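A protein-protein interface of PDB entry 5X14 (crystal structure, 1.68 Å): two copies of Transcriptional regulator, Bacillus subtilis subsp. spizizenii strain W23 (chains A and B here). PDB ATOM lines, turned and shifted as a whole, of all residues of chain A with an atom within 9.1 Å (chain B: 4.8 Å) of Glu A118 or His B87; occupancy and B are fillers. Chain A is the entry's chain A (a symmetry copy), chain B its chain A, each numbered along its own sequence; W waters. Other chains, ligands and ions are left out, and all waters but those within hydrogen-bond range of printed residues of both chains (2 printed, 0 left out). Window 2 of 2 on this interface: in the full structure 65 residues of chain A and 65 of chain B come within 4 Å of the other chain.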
ATOM      1  N   PHE A 104      -1.749 -28.468  23.481  1.00  0.00           N
ATOM      2  CA  PHE A 104      -0.454 -29.142  23.517  1.00  0.00           C
ATOM      3  C   PHE A 104       0.495 -28.476  22.506  1.00  0.00           C
ATOM      4  O   PHE A 104       1.668 -28.334  22.739  1.00  0.00           O
ATOM      5  CB  PHE A 104      -0.571 -30.687  23.208  1.00  0.00           C
ATOM      6  CG  PHE A 104       0.771 -31.365  23.147  1.00  0.00           C
ATOM      7  CD1 PHE A 104       1.459 -31.693  24.305  1.00  0.00           C
ATOM      8  CD2 PHE A 104       1.410 -31.569  21.931  1.00  0.00           C
ATOM      9  CE1 PHE A 104       2.735 -32.246  24.264  1.00  0.00           C
ATOM     10  CE2 PHE A 104       2.700 -32.098  21.919  1.00  0.00           C
ATOM     11  CZ  PHE A 104       3.324 -32.434  23.060  1.00  0.00           C
ATOM     12  N   LYS A 107       2.058 -25.388  23.767  1.00  0.00           N
ATOM     13  CA  LYS A 107       3.177 -25.746  24.600  1.00  0.00           C
ATOM     14  C   LYS A 107       4.401 -26.031  23.756  1.00  0.00           C
ATOM     15  O   LYS A 107       5.487 -25.546  24.056  1.00  0.00           O
ATOM     16  CB  LYS A 107       2.853 -26.937  25.495  1.00  0.00           C
ATOM     17  CG  LYS A 107       1.696 -26.681  26.523  1.00  0.00           C
ATOM     18  CD  LYS A 107       1.606 -27.883  27.460  1.00  0.00           C
ATOM     19  CE  LYS A 107       0.498 -27.815  28.477  1.00  0.00           C
ATOM     20  NZ  LYS A 107       0.770 -29.029  29.414  1.00  0.00           N
ATOM     21  N   PHE A 110       6.326 -23.090  22.608  1.00  0.00           N
ATOM     22  CA  PHE A 110       7.086 -22.489  23.682  1.00  0.00           C
ATOM     23  C   PHE A 110       8.127 -23.432  24.325  1.00  0.00           C
ATOM     24  O   PHE A 110       8.596 -23.210  25.462  1.00  0.00           O
ATOM     25  CB  PHE A 110       6.078 -21.948  24.727  1.00  0.00           C
ATOM     26  CG  PHE A 110       5.208 -20.842  24.188  1.00  0.00           C
ATOM     27  CD1 PHE A 110       5.754 -19.803  23.430  1.00  0.00           C
ATOM     28  CD2 PHE A 110       3.821 -20.848  24.401  1.00  0.00           C
ATOM     29  CE1 PHE A 110       4.976 -18.769  22.925  1.00  0.00           C
ATOM     30  CE2 PHE A 110       3.034 -19.818  23.883  1.00  0.00           C
ATOM     31  CZ  PHE A 110       3.581 -18.800  23.139  1.00  0.00           C
ATOM     32  N   ILE A 111       8.452 -24.502  23.605  1.00  0.00           N
ATOM     33  CA  ILE A 111       9.386 -25.552  24.088  1.00  0.00           C
ATOM     34  C   ILE A 111      10.725 -24.997  24.579  1.00  0.00           C
ATOM     35  O   ILE A 111      11.422 -25.638  25.406  1.00  0.00           O
ATOM     36  CB  ILE A 111       9.620 -26.648  22.988  1.00  0.00           C
ATOM     37  CG1 ILE A 111      10.211 -27.929  23.614  1.00  0.00           C
ATOM     38  CG2 ILE A 111      10.424 -26.067  21.771  1.00  0.00           C
ATOM     39  CD1 ILE A 111      10.306 -29.110  22.674  1.00  0.00           C
ATOM     40  N   SER A 112      11.124 -23.812  24.109  1.00  0.00           N
ATOM     41  CA  SER A 112      12.390 -23.188  24.558  1.00  0.00           C
ATOM     42  C   SER A 112      12.411 -22.958  26.080  1.00  0.00           C
ATOM     43  O   SER A 112      13.492 -22.906  26.680  1.00  0.00           O
ATOM     44  CB  SER A 112      12.720 -21.874  23.854  1.00  0.00           C
ATOM     45  OG  SER A 112      11.897 -20.787  24.284  1.00  0.00           O
ATOM     46  N   SER A 113      11.238 -22.892  26.706  1.00  0.00           N
ATOM     47  CA  SER A 113      11.177 -22.716  28.156  1.00  0.00           C
ATOM     48  C   SER A 113      11.364 -24.018  28.962  1.00  0.00           C
ATOM     49  O   SER A 113      11.333 -23.970  30.195  1.00  0.00           O
ATOM     50  CB  SER A 113       9.861 -22.027  28.535  1.00  0.00           C
ATOM     51  OG  SER A 113       9.901 -20.629  28.199  1.00  0.00           O
ATOM     52  N   LEU A 114      11.591 -25.159  28.284  1.00  0.00           N
ATOM     53  CA  LEU A 114      11.826 -26.479  28.909  1.00  0.00           C
ATOM     54  C   LEU A 114      13.214 -27.023  28.613  1.00  0.00           C
ATOM     55  O   LEU A 114      13.754 -26.821  27.524  1.00  0.00           O
ATOM     56  CB  LEU A 114      10.805 -27.515  28.387  1.00  0.00           C
ATOM     57  CG  LEU A 114       9.335 -27.182  28.675  1.00  0.00           C
ATOM     58  CD1 LEU A 114       8.394 -28.235  28.025  1.00  0.00           C
ATOM     59  CD2 LEU A 114       9.017 -27.042  30.131  1.00  0.00           C
ATOM     60  N   SER A 115      13.798 -27.695  29.606  1.00  0.00           N
ATOM     61  CA  SER A 115      15.030 -28.448  29.411  1.00  0.00           C
ATOM     62  C   SER A 115      14.791 -29.625  28.476  1.00  0.00           C
ATOM     63  O   SER A 115      13.651 -30.000  28.221  1.00  0.00           O
ATOM     64  CB  SER A 115      15.568 -28.967  30.747  1.00  0.00           C
ATOM     65  OG  SER A 115      14.715 -29.963  31.259  1.00  0.00           O
ATOM     66  N   ARG A 116      15.865 -30.216  27.959  1.00  0.00           N
ATOM     67  CA  ARG A 116      15.701 -31.427  27.123  1.00  0.00           C
ATOM     68  C   ARG A 116      14.905 -32.528  27.859  1.00  0.00           C
ATOM     69  O   ARG A 116      14.023 -33.196  27.277  1.00  0.00           O
ATOM     70  CB  ARG A 116      17.099 -31.939  26.678  1.00  0.00           C
ATOM     71  CG  ARG A 116      17.064 -33.036  25.584  1.00  0.00           C
ATOM     72  CD  ARG A 116      18.470 -33.579  25.197  1.00  0.00           C
ATOM     73  NE  ARG A 116      19.411 -32.563  24.679  1.00  0.00           N
ATOM     74  CZ  ARG A 116      19.561 -32.200  23.397  1.00  0.00           C
ATOM     75  NH1 ARG A 116      18.829 -32.719  22.406  1.00  0.00           N
ATOM     76  NH2 ARG A 116      20.455 -31.264  23.085  1.00  0.00           N
ATOM     77  N   GLN A 117      15.193 -32.735  29.137  1.00  0.00           N
ATOM     78  CA  GLN A 117      14.472 -33.749  29.888  1.00  0.00           C
ATOM     79  C   GLN A 117      13.029 -33.363  30.088  1.00  0.00           C
ATOM     80  O   GLN A 117      12.148 -34.206  29.960  1.00  0.00           O
ATOM     81  CB  GLN A 117      15.128 -34.032  31.249  1.00  0.00           C
ATOM     82  CG  GLN A 117      14.499 -35.236  31.997  1.00  0.00           C
ATOM     83  CD  GLN A 117      14.632 -36.575  31.237  1.00  0.00           C
ATOM     84  OE1 GLN A 117      15.751 -37.020  30.915  1.00  0.00           O
ATOM     85  NE2 GLN A 117      13.486 -37.217  30.933  1.00  0.00           N
ATOM     86  N   GLU A 118      12.775 -32.099  30.429  1.00  0.00           N
ATOM     87  CA  GLU A 118      11.374 -31.652  30.579  1.00  0.00           C
ATOM     88  C   GLU A 118      10.581 -31.803  29.296  1.00  0.00           C
ATOM     89  O   GLU A 118       9.398 -32.219  29.325  1.00  0.00           O
ATOM     90  CB  GLU A 118      11.311 -30.226  31.050  1.00  0.00           C
ATOM     91  CG  GLU A 118      11.629 -30.067  32.471  1.00  0.00           C
ATOM     92  CD  GLU A 118      11.869 -28.617  32.878  1.00  0.00           C
ATOM     93  OE1 GLU A 118      12.307 -27.763  32.044  1.00  0.00           O
ATOM     94  OE2 GLU A 118      11.683 -28.353  34.079  1.00  0.00           O
ATOM     95  N   ALA A 119      11.224 -31.500  28.173  1.00  0.00           N
ATOM     96  CA  ALA A 119      10.599 -31.622  26.859  1.00  0.00           C
ATOM     97  C   ALA A 119      10.330 -33.090  26.583  1.00  0.00           C
ATOM     98  O   ALA A 119       9.242 -33.442  26.137  1.00  0.00           O
ATOM     99  CB  ALA A 119      11.461 -30.981  25.761  1.00  0.00           C
ATOM    100  N   SER A 120      11.316 -33.942  26.855  1.00  0.00           N
ATOM    101  CA  SER A 120      11.122 -35.386  26.677  1.00  0.00           C
ATOM    102  C   SER A 120       9.925 -35.877  27.499  1.00  0.00           C
ATOM    103  O   SER A 120       9.112 -36.646  27.000  1.00  0.00           O
ATOM    104  CB  SER A 120      12.366 -36.155  27.103  1.00  0.00           C
ATOM    105  OG  SER A 120      12.189 -37.541  26.805  1.00  0.00           O
ATOM    106  N   ASP A 121       9.793 -35.423  28.751  1.00  0.00           N
ATOM    107  CA  ASP A 121       8.729 -35.931  29.616  1.00  0.00           C
ATOM    108  C   ASP A 121       7.359 -35.459  29.137  1.00  0.00           C
ATOM    109  O   ASP A 121       6.367 -36.216  29.192  1.00  0.00           O
ATOM    110  CB  ASP A 121       8.995 -35.545  31.066  1.00  0.00           C
ATOM    111  CG  ASP A 121      10.200 -36.294  31.671  1.00  0.00           C
ATOM    112  OD1 ASP A 121      10.638 -37.352  31.142  1.00  0.00           O
ATOM    113  OD2 ASP A 121      10.707 -35.825  32.700  1.00  0.00           O
ATOM    114  N   LEU A 122       7.303 -34.210  28.685  1.00  0.00           N
ATOM    115  CA  LEU A 122       6.046 -33.645  28.146  1.00  0.00           C
ATOM    116  C   LEU A 122       5.592 -34.400  26.921  1.00  0.00           C
ATOM    117  O   LEU A 122       4.407 -34.787  26.809  1.00  0.00           O
ATOM    118  CB  LEU A 122       6.204 -32.165  27.847  1.00  0.00           C
ATOM    119  CG  LEU A 122       5.034 -31.444  27.162  1.00  0.00           C
ATOM    120  CD1 LEU A 122       3.829 -31.522  28.094  1.00  0.00           C
ATOM    121  CD2 LEU A 122       5.424 -30.025  26.740  1.00  0.00           C
ATOM    122  N   PHE A 123       6.517 -34.612  25.987  1.00  0.00           N
ATOM    123  CA  PHE A 123       6.171 -35.279  24.730  1.00  0.00           C
ATOM    124  C   PHE A 123       5.846 -36.779  24.927  1.00  0.00           C
ATOM    125  O   PHE A 123       4.973 -37.299  24.272  1.00  0.00           O
ATOM    126  CB  PHE A 123       7.264 -35.078  23.652  1.00  0.00           C
ATOM    127  CG  PHE A 123       7.097 -33.808  22.879  1.00  0.00           C
ATOM    128  CD1 PHE A 123       7.246 -32.595  23.520  1.00  0.00           C
ATOM    129  CD2 PHE A 123       6.648 -33.849  21.554  1.00  0.00           C
ATOM    130  CE1 PHE A 123       7.046 -31.422  22.837  1.00  0.00           C
ATOM    131  CE2 PHE A 123       6.432 -32.664  20.876  1.00  0.00           C
ATOM    132  CZ  PHE A 123       6.626 -31.474  21.536  1.00  0.00           C
ATOM    133  N   THR A 124       6.534 -37.414  25.862  1.00  0.00           N
ATOM    134  CA  THR A 124       6.345 -38.836  26.150  1.00  0.00           C
ATOM    135  C   THR A 124       4.970 -39.003  26.782  1.00  0.00           C
ATOM    136  O   THR A 124       4.251 -39.893  26.412  1.00  0.00           O
ATOM    137  CB  THR A 124       7.393 -39.366  27.097  1.00  0.00           C
ATOM    138  OG1 THR A 124       8.719 -39.268  26.532  1.00  0.00           O
ATOM    139  CG2 THR A 124       7.118 -40.818  27.506  1.00  0.00           C
ATOM    140  N   ASP A 125       4.598 -38.118  27.710  1.00  0.00           N
ATOM    141  CA  ASP A 125       3.195 -38.134  28.275  1.00  0.00           C
ATOM    142  C   ASP A 125       2.142 -38.040  27.175  1.00  0.00           C
ATOM    143  O   ASP A 125       1.181 -38.843  27.145  1.00  0.00           O
ATOM    144  CB  ASP A 125       3.002 -36.982  29.302  1.00  0.00           C
ATOM    145  CG  ASP A 125       1.593 -36.938  29.850  1.00  0.00           C
ATOM    146  OD1 ASP A 125       1.242 -37.790  30.708  1.00  0.00           O
ATOM    147  OD2 ASP A 125       0.822 -36.132  29.334  1.00  0.00           O
ATOM    148  N   LEU A 182      10.267 -36.819  19.554  1.00  0.00           N
ATOM    149  CA  LEU A 182      10.994 -37.492  20.628  1.00  0.00           C
ATOM    150  C   LEU A 182      12.385 -37.937  20.136  1.00  0.00           C
ATOM    151  O   LEU A 182      13.360 -37.797  20.860  1.00  0.00           O
ATOM    152  CB  LEU A 182      10.213 -38.679  21.173  1.00  0.00           C
ATOM    153  CG  LEU A 182       9.083 -38.291  22.143  1.00  0.00           C
ATOM    154  CD1 LEU A 182       8.050 -39.436  22.375  1.00  0.00           C
ATOM    155  CD2 LEU A 182       9.622 -37.734  23.517  1.00  0.00           C
ATOM    156  N   ILE A 185      14.438 -34.880  20.095  1.00  0.00           N
ATOM    157  CA  ILE A 185      14.789 -34.491  21.481  1.00  0.00           C
ATOM    158  C   ILE A 185      15.917 -35.429  21.953  1.00  0.00           C
ATOM    159  O   ILE A 185      16.875 -34.953  22.580  1.00  0.00           O
ATOM    160  CB  ILE A 185      13.563 -34.523  22.429  1.00  0.00           C
ATOM    161  CG1 ILE A 185      12.571 -33.408  22.077  1.00  0.00           C
ATOM    162  CG2 ILE A 185      13.976 -34.330  23.894  1.00  0.00           C
ATOM    163  CD1 ILE A 185      11.162 -33.604  22.641  1.00  0.00           C
ATOM    164  N   LYS B  83       6.823 -16.152  34.914  1.00  0.00           N
ATOM    165  CA  LYS B  83       7.667 -17.286  34.526  1.00  0.00           C
ATOM    166  C   LYS B  83       7.219 -18.596  35.195  1.00  0.00           C
ATOM    167  O   LYS B  83       7.155 -19.636  34.547  1.00  0.00           O
ATOM    168  CB  LYS B  83       9.132 -17.001  34.855  1.00  0.00           C
ATOM    169  CG  LYS B  83       9.742 -15.914  34.039  1.00  0.00           C
ATOM    170  CD  LYS B  83      11.228 -15.738  34.296  1.00  0.00           C
ATOM    171  CE  LYS B  83      11.749 -14.494  33.560  1.00  0.00           C
ATOM    172  NZ  LYS B  83      13.075 -14.061  34.045  1.00  0.00           N
ATOM    173  N   GLN B  84       6.844 -18.532  36.462  1.00  0.00           N
ATOM    174  CA  GLN B  84       6.383 -19.701  37.193  1.00  0.00           C
ATOM    175  C   GLN B  84       5.016 -20.135  36.669  1.00  0.00           C
ATOM    176  O   GLN B  84       4.725 -21.341  36.541  1.00  0.00           O
ATOM    177  CB  GLN B  84       6.287 -19.420  38.704  1.00  0.00           C
ATOM    178  CG  GLN B  84       6.023 -20.703  39.548  1.00  0.00           C
ATOM    179  CD  GLN B  84       7.188 -21.698  39.520  1.00  0.00           C
ATOM    180  OE1 GLN B  84       8.340 -21.324  39.826  1.00  0.00           O
ATOM    181  NE2 GLN B  84       6.903 -22.974  39.155  1.00  0.00           N
ATOM    182  N   GLU B  85       4.188 -19.154  36.348  1.00  0.00           N
ATOM    183  CA  GLU B  85       2.838 -19.445  35.829  1.00  0.00           C
ATOM    184  C   GLU B  85       2.939 -20.186  34.491  1.00  0.00           C
ATOM    185  O   GLU B  85       2.286 -21.226  34.267  1.00  0.00           O
ATOM    186  CB  GLU B  85       2.014 -18.155  35.723  1.00  0.00           C
ATOM    187  CG  GLU B  85       0.485 -18.348  35.478  1.00  0.00           C
ATOM    188  CD  GLU B  85      -0.333 -18.715  36.698  1.00  0.00           C
ATOM    189  OE1 GLU B  85       0.212 -18.973  37.815  1.00  0.00           O
ATOM    190  OE2 GLU B  85      -1.588 -18.759  36.582  1.00  0.00           O
ATOM    191  N   LEU B  86       3.815 -19.699  33.618  1.00  0.00           N
ATOM    192  CA  LEU B  86       4.052 -20.384  32.315  1.00  0.00           C
ATOM    193  C   LEU B  86       4.671 -21.781  32.504  1.00  0.00           C
ATOM    194  O   LEU B  86       4.324 -22.750  31.833  1.00  0.00           O
ATOM    195  CB  LEU B  86       4.988 -19.503  31.478  1.00  0.00           C
ATOM    196  CG  LEU B  86       5.452 -20.051  30.153  1.00  0.00           C
ATOM    197  CD1 LEU B  86       4.237 -20.139  29.192  1.00  0.00           C
ATOM    198  CD2 LEU B  86       6.581 -19.223  29.597  1.00  0.00           C
ATOM    199  N   HIS B  87       5.636 -21.878  33.403  1.00  0.00           N
ATOM    200  CA  HIS B  87       6.310 -23.166  33.645  1.00  0.00           C
ATOM    201  C   HIS B  87       5.312 -24.235  34.151  1.00  0.00           C
ATOM    202  O   HIS B  87       5.307 -25.374  33.654  1.00  0.00           O
ATOM    203  CB  HIS B  87       7.451 -22.970  34.657  1.00  0.00           C
ATOM    204  CG  HIS B  87       8.132 -24.244  35.052  1.00  0.00           C
ATOM    205  ND1 HIS B  87       9.074 -24.861  34.252  1.00  0.00           N
ATOM    206  CD2 HIS B  87       7.969 -25.051  36.129  1.00  0.00           C
ATOM    207  CE1 HIS B  87       9.478 -25.977  34.830  1.00  0.00           C
ATOM    208  NE2 HIS B  87       8.839 -26.106  35.981  1.00  0.00           N
ATOM    209  N   ASP B  88       4.487 -23.869  35.136  1.00  0.00           N
ATOM    210  CA  ASP B  88       3.513 -24.813  35.719  1.00  0.00           C
ATOM    211  C   ASP B  88       2.547 -25.344  34.647  1.00  0.00           C
ATOM    212  O   ASP B  88       2.181 -26.514  34.630  1.00  0.00           O
ATOM    213  CB  ASP B  88       2.722 -24.148  36.852  1.00  0.00           C
ATOM    214  CG  ASP B  88       3.583 -23.859  38.105  1.00  0.00           C
ATOM    215  OD1 ASP B  88       4.717 -24.387  38.249  1.00  0.00           O
ATOM    216  OD2 ASP B  88       3.117 -23.037  38.940  1.00  0.00           O
ATOM    217  N   TRP B  89       2.087 -24.443  33.778  1.00  0.00           N
ATOM    218  CA  TRP B  89       1.176 -24.829  32.668  1.00  0.00           C
ATOM    219  C   TRP B  89       1.869 -25.748  31.662  1.00  0.00           C
ATOM    220  O   TRP B  89       1.277 -26.728  31.213  1.00  0.00           O
ATOM    221  CB  TRP B  89       0.663 -23.549  31.975  1.00  0.00           C
ATOM    222  CG  TRP B  89      -0.028 -23.773  30.663  1.00  0.00           C
ATOM    223  CD1 TRP B  89      -1.308 -24.119  30.470  1.00  0.00           C
ATOM    224  CD2 TRP B  89       0.511 -23.475  29.372  1.00  0.00           C
ATOM    225  NE1 TRP B  89      -1.588 -24.184  29.116  1.00  0.00           N
ATOM    226  CE2 TRP B  89      -0.470 -23.803  28.428  1.00  0.00           C
ATOM    227  CE3 TRP B  89       1.751 -23.073  28.920  1.00  0.00           C
ATOM    228  CZ2 TRP B  89      -0.267 -23.659  27.071  1.00  0.00           C
ATOM    229  CZ3 TRP B  89       1.946 -22.931  27.562  1.00  0.00           C
ATOM    230  CH2 TRP B  89       0.943 -23.217  26.659  1.00  0.00           C
ATOM    231  N   LEU B  90       3.118 -25.434  31.307  1.00  0.00           N
ATOM    232  CA  LEU B  90       3.870 -26.246  30.338  1.00  0.00           C
ATOM    233  C   LEU B  90       4.023 -27.679  30.845  1.00  0.00           C
ATOM    234  O   LEU B  90       3.860 -28.617  30.104  1.00  0.00           O
ATOM    235  CB  LEU B  90       5.303 -25.688  30.055  1.00  0.00           C
ATOM    236  CG  LEU B  90       5.393 -24.432  29.167  1.00  0.00           C
ATOM    237  CD1 LEU B  90       6.771 -23.698  29.262  1.00  0.00           C
ATOM    238  CD2 LEU B  90       5.019 -24.781  27.695  1.00  0.00           C
ATOM    239  N   ILE B  91       4.356 -27.834  32.119  1.00  0.00           N
ATOM    240  CA  ILE B  91       4.610 -29.189  32.624  1.00  0.00           C
ATOM    241  C   ILE B  91       3.401 -29.975  33.167  1.00  0.00           C
ATOM    242  O   ILE B  91       3.505 -31.200  33.384  1.00  0.00           O
ATOM    243  CB  ILE B  91       5.739 -29.201  33.652  1.00  0.00           C
ATOM    244  CG1 ILE B  91       5.299 -28.543  34.937  1.00  0.00           C
ATOM    245  CG2 ILE B  91       7.024 -28.539  33.068  1.00  0.00           C
ATOM    246  CD1 ILE B  91       6.294 -28.925  36.096  1.00  0.00           C
HETATM  247  O   HOH W   1      11.881 -25.307  32.584  1.00  0.00           O
HETATM  248  O   HOH W   2       9.361 -23.138  32.083  1.00  0.00           O
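The side-chain amino group (NZ) of Lys A107 lies within hydrogen-bond range of the backbone carbonyl oxygen (O) of Trp B89.
O of Leu B90 is in hydrogen-bond range of NZ of Lys A107, at 3.2 Å.
Ser A113 touches Leu B86.
Ser A113 touches Leu B90 (CB to CD1, 3.6 Å).
Leu A114 touches Leu B90.
CD2 of Leu A114 touches CG2 of Ile B91 (3.9 Å).
CE1 of His B87 touches OE2 of Glu A118, 3.3 Å away.
CD1 of Leu A122 touches O of Leu B90, 3.5 Å away.
No position is printed for both chains.
Of the 8 pairs that touch across the chains among the printed residues, none has its exchanged pair printed and touching as well.
N of Ser A115 lies within hydrogen-bond range of OE1 of Glu A118, 2.9 Å away.
Printed residues of chain B within 4 Å of Lys A107: Trp B89 and Leu B90.
Of the printed residues of chain B, Ser A113 touches Leu B86 and Leu B90.
Glu A118 touches just one residue of chain B: His B87 (3.3 Å).
Of the printed residues of chain B, Leu A122 touches Leu B90 (3.5 Å).
Lys B83 touches none of the printed residues of chain A.
Leu B86 touches just one residue of chain A: Ser A113.
Printed residues of chain A within 4 Å of His B87: Glu A118 (3.3 Å).
Of the printed residues of chain A, Trp B89 touches Lys A107 (3.0 Å).
Printed residues of chain A within 4 Å of Leu B90: Lys A107 (3.2 Å), Ser A113 (3.6 Å), Leu A114 (3.95 Å) and Leu A122 (3.5 Å).
The nearest residue of chain A that does not touch His B87 is Leu A114 (4.7 Å).
Water W1 lies within hydrogen-bond range of OE1 of Glu A118 (2.6 Å), O of Ser A113 (2.8 Å) and ND1 of His B87 (3.3 Å).
Water W2 lies within hydrogen-bond range of a ring nitrogen (ND1) of His B87 (2.8 Å) and the backbone carbonyl oxygen (O) of Ser A113 (2.9 Å).
Of the 20 printed residues of chain A, 5 touch a printed residue of chain B.
Hydrophobic or aromatic side chains of chain A that line the printed part of chain B: Leu A114 and Leu A122.
Of the 9 printed residues of chain B, 5 touch a printed residue of chain A.
Hydrophobic or aromatic side chains of chain B within 4 Å of the printed part of chain A: Leu B86, His B87, Trp B89, Leu B90 and Ile B91.
Among the printed residues, 8 pairs touch across the chains.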
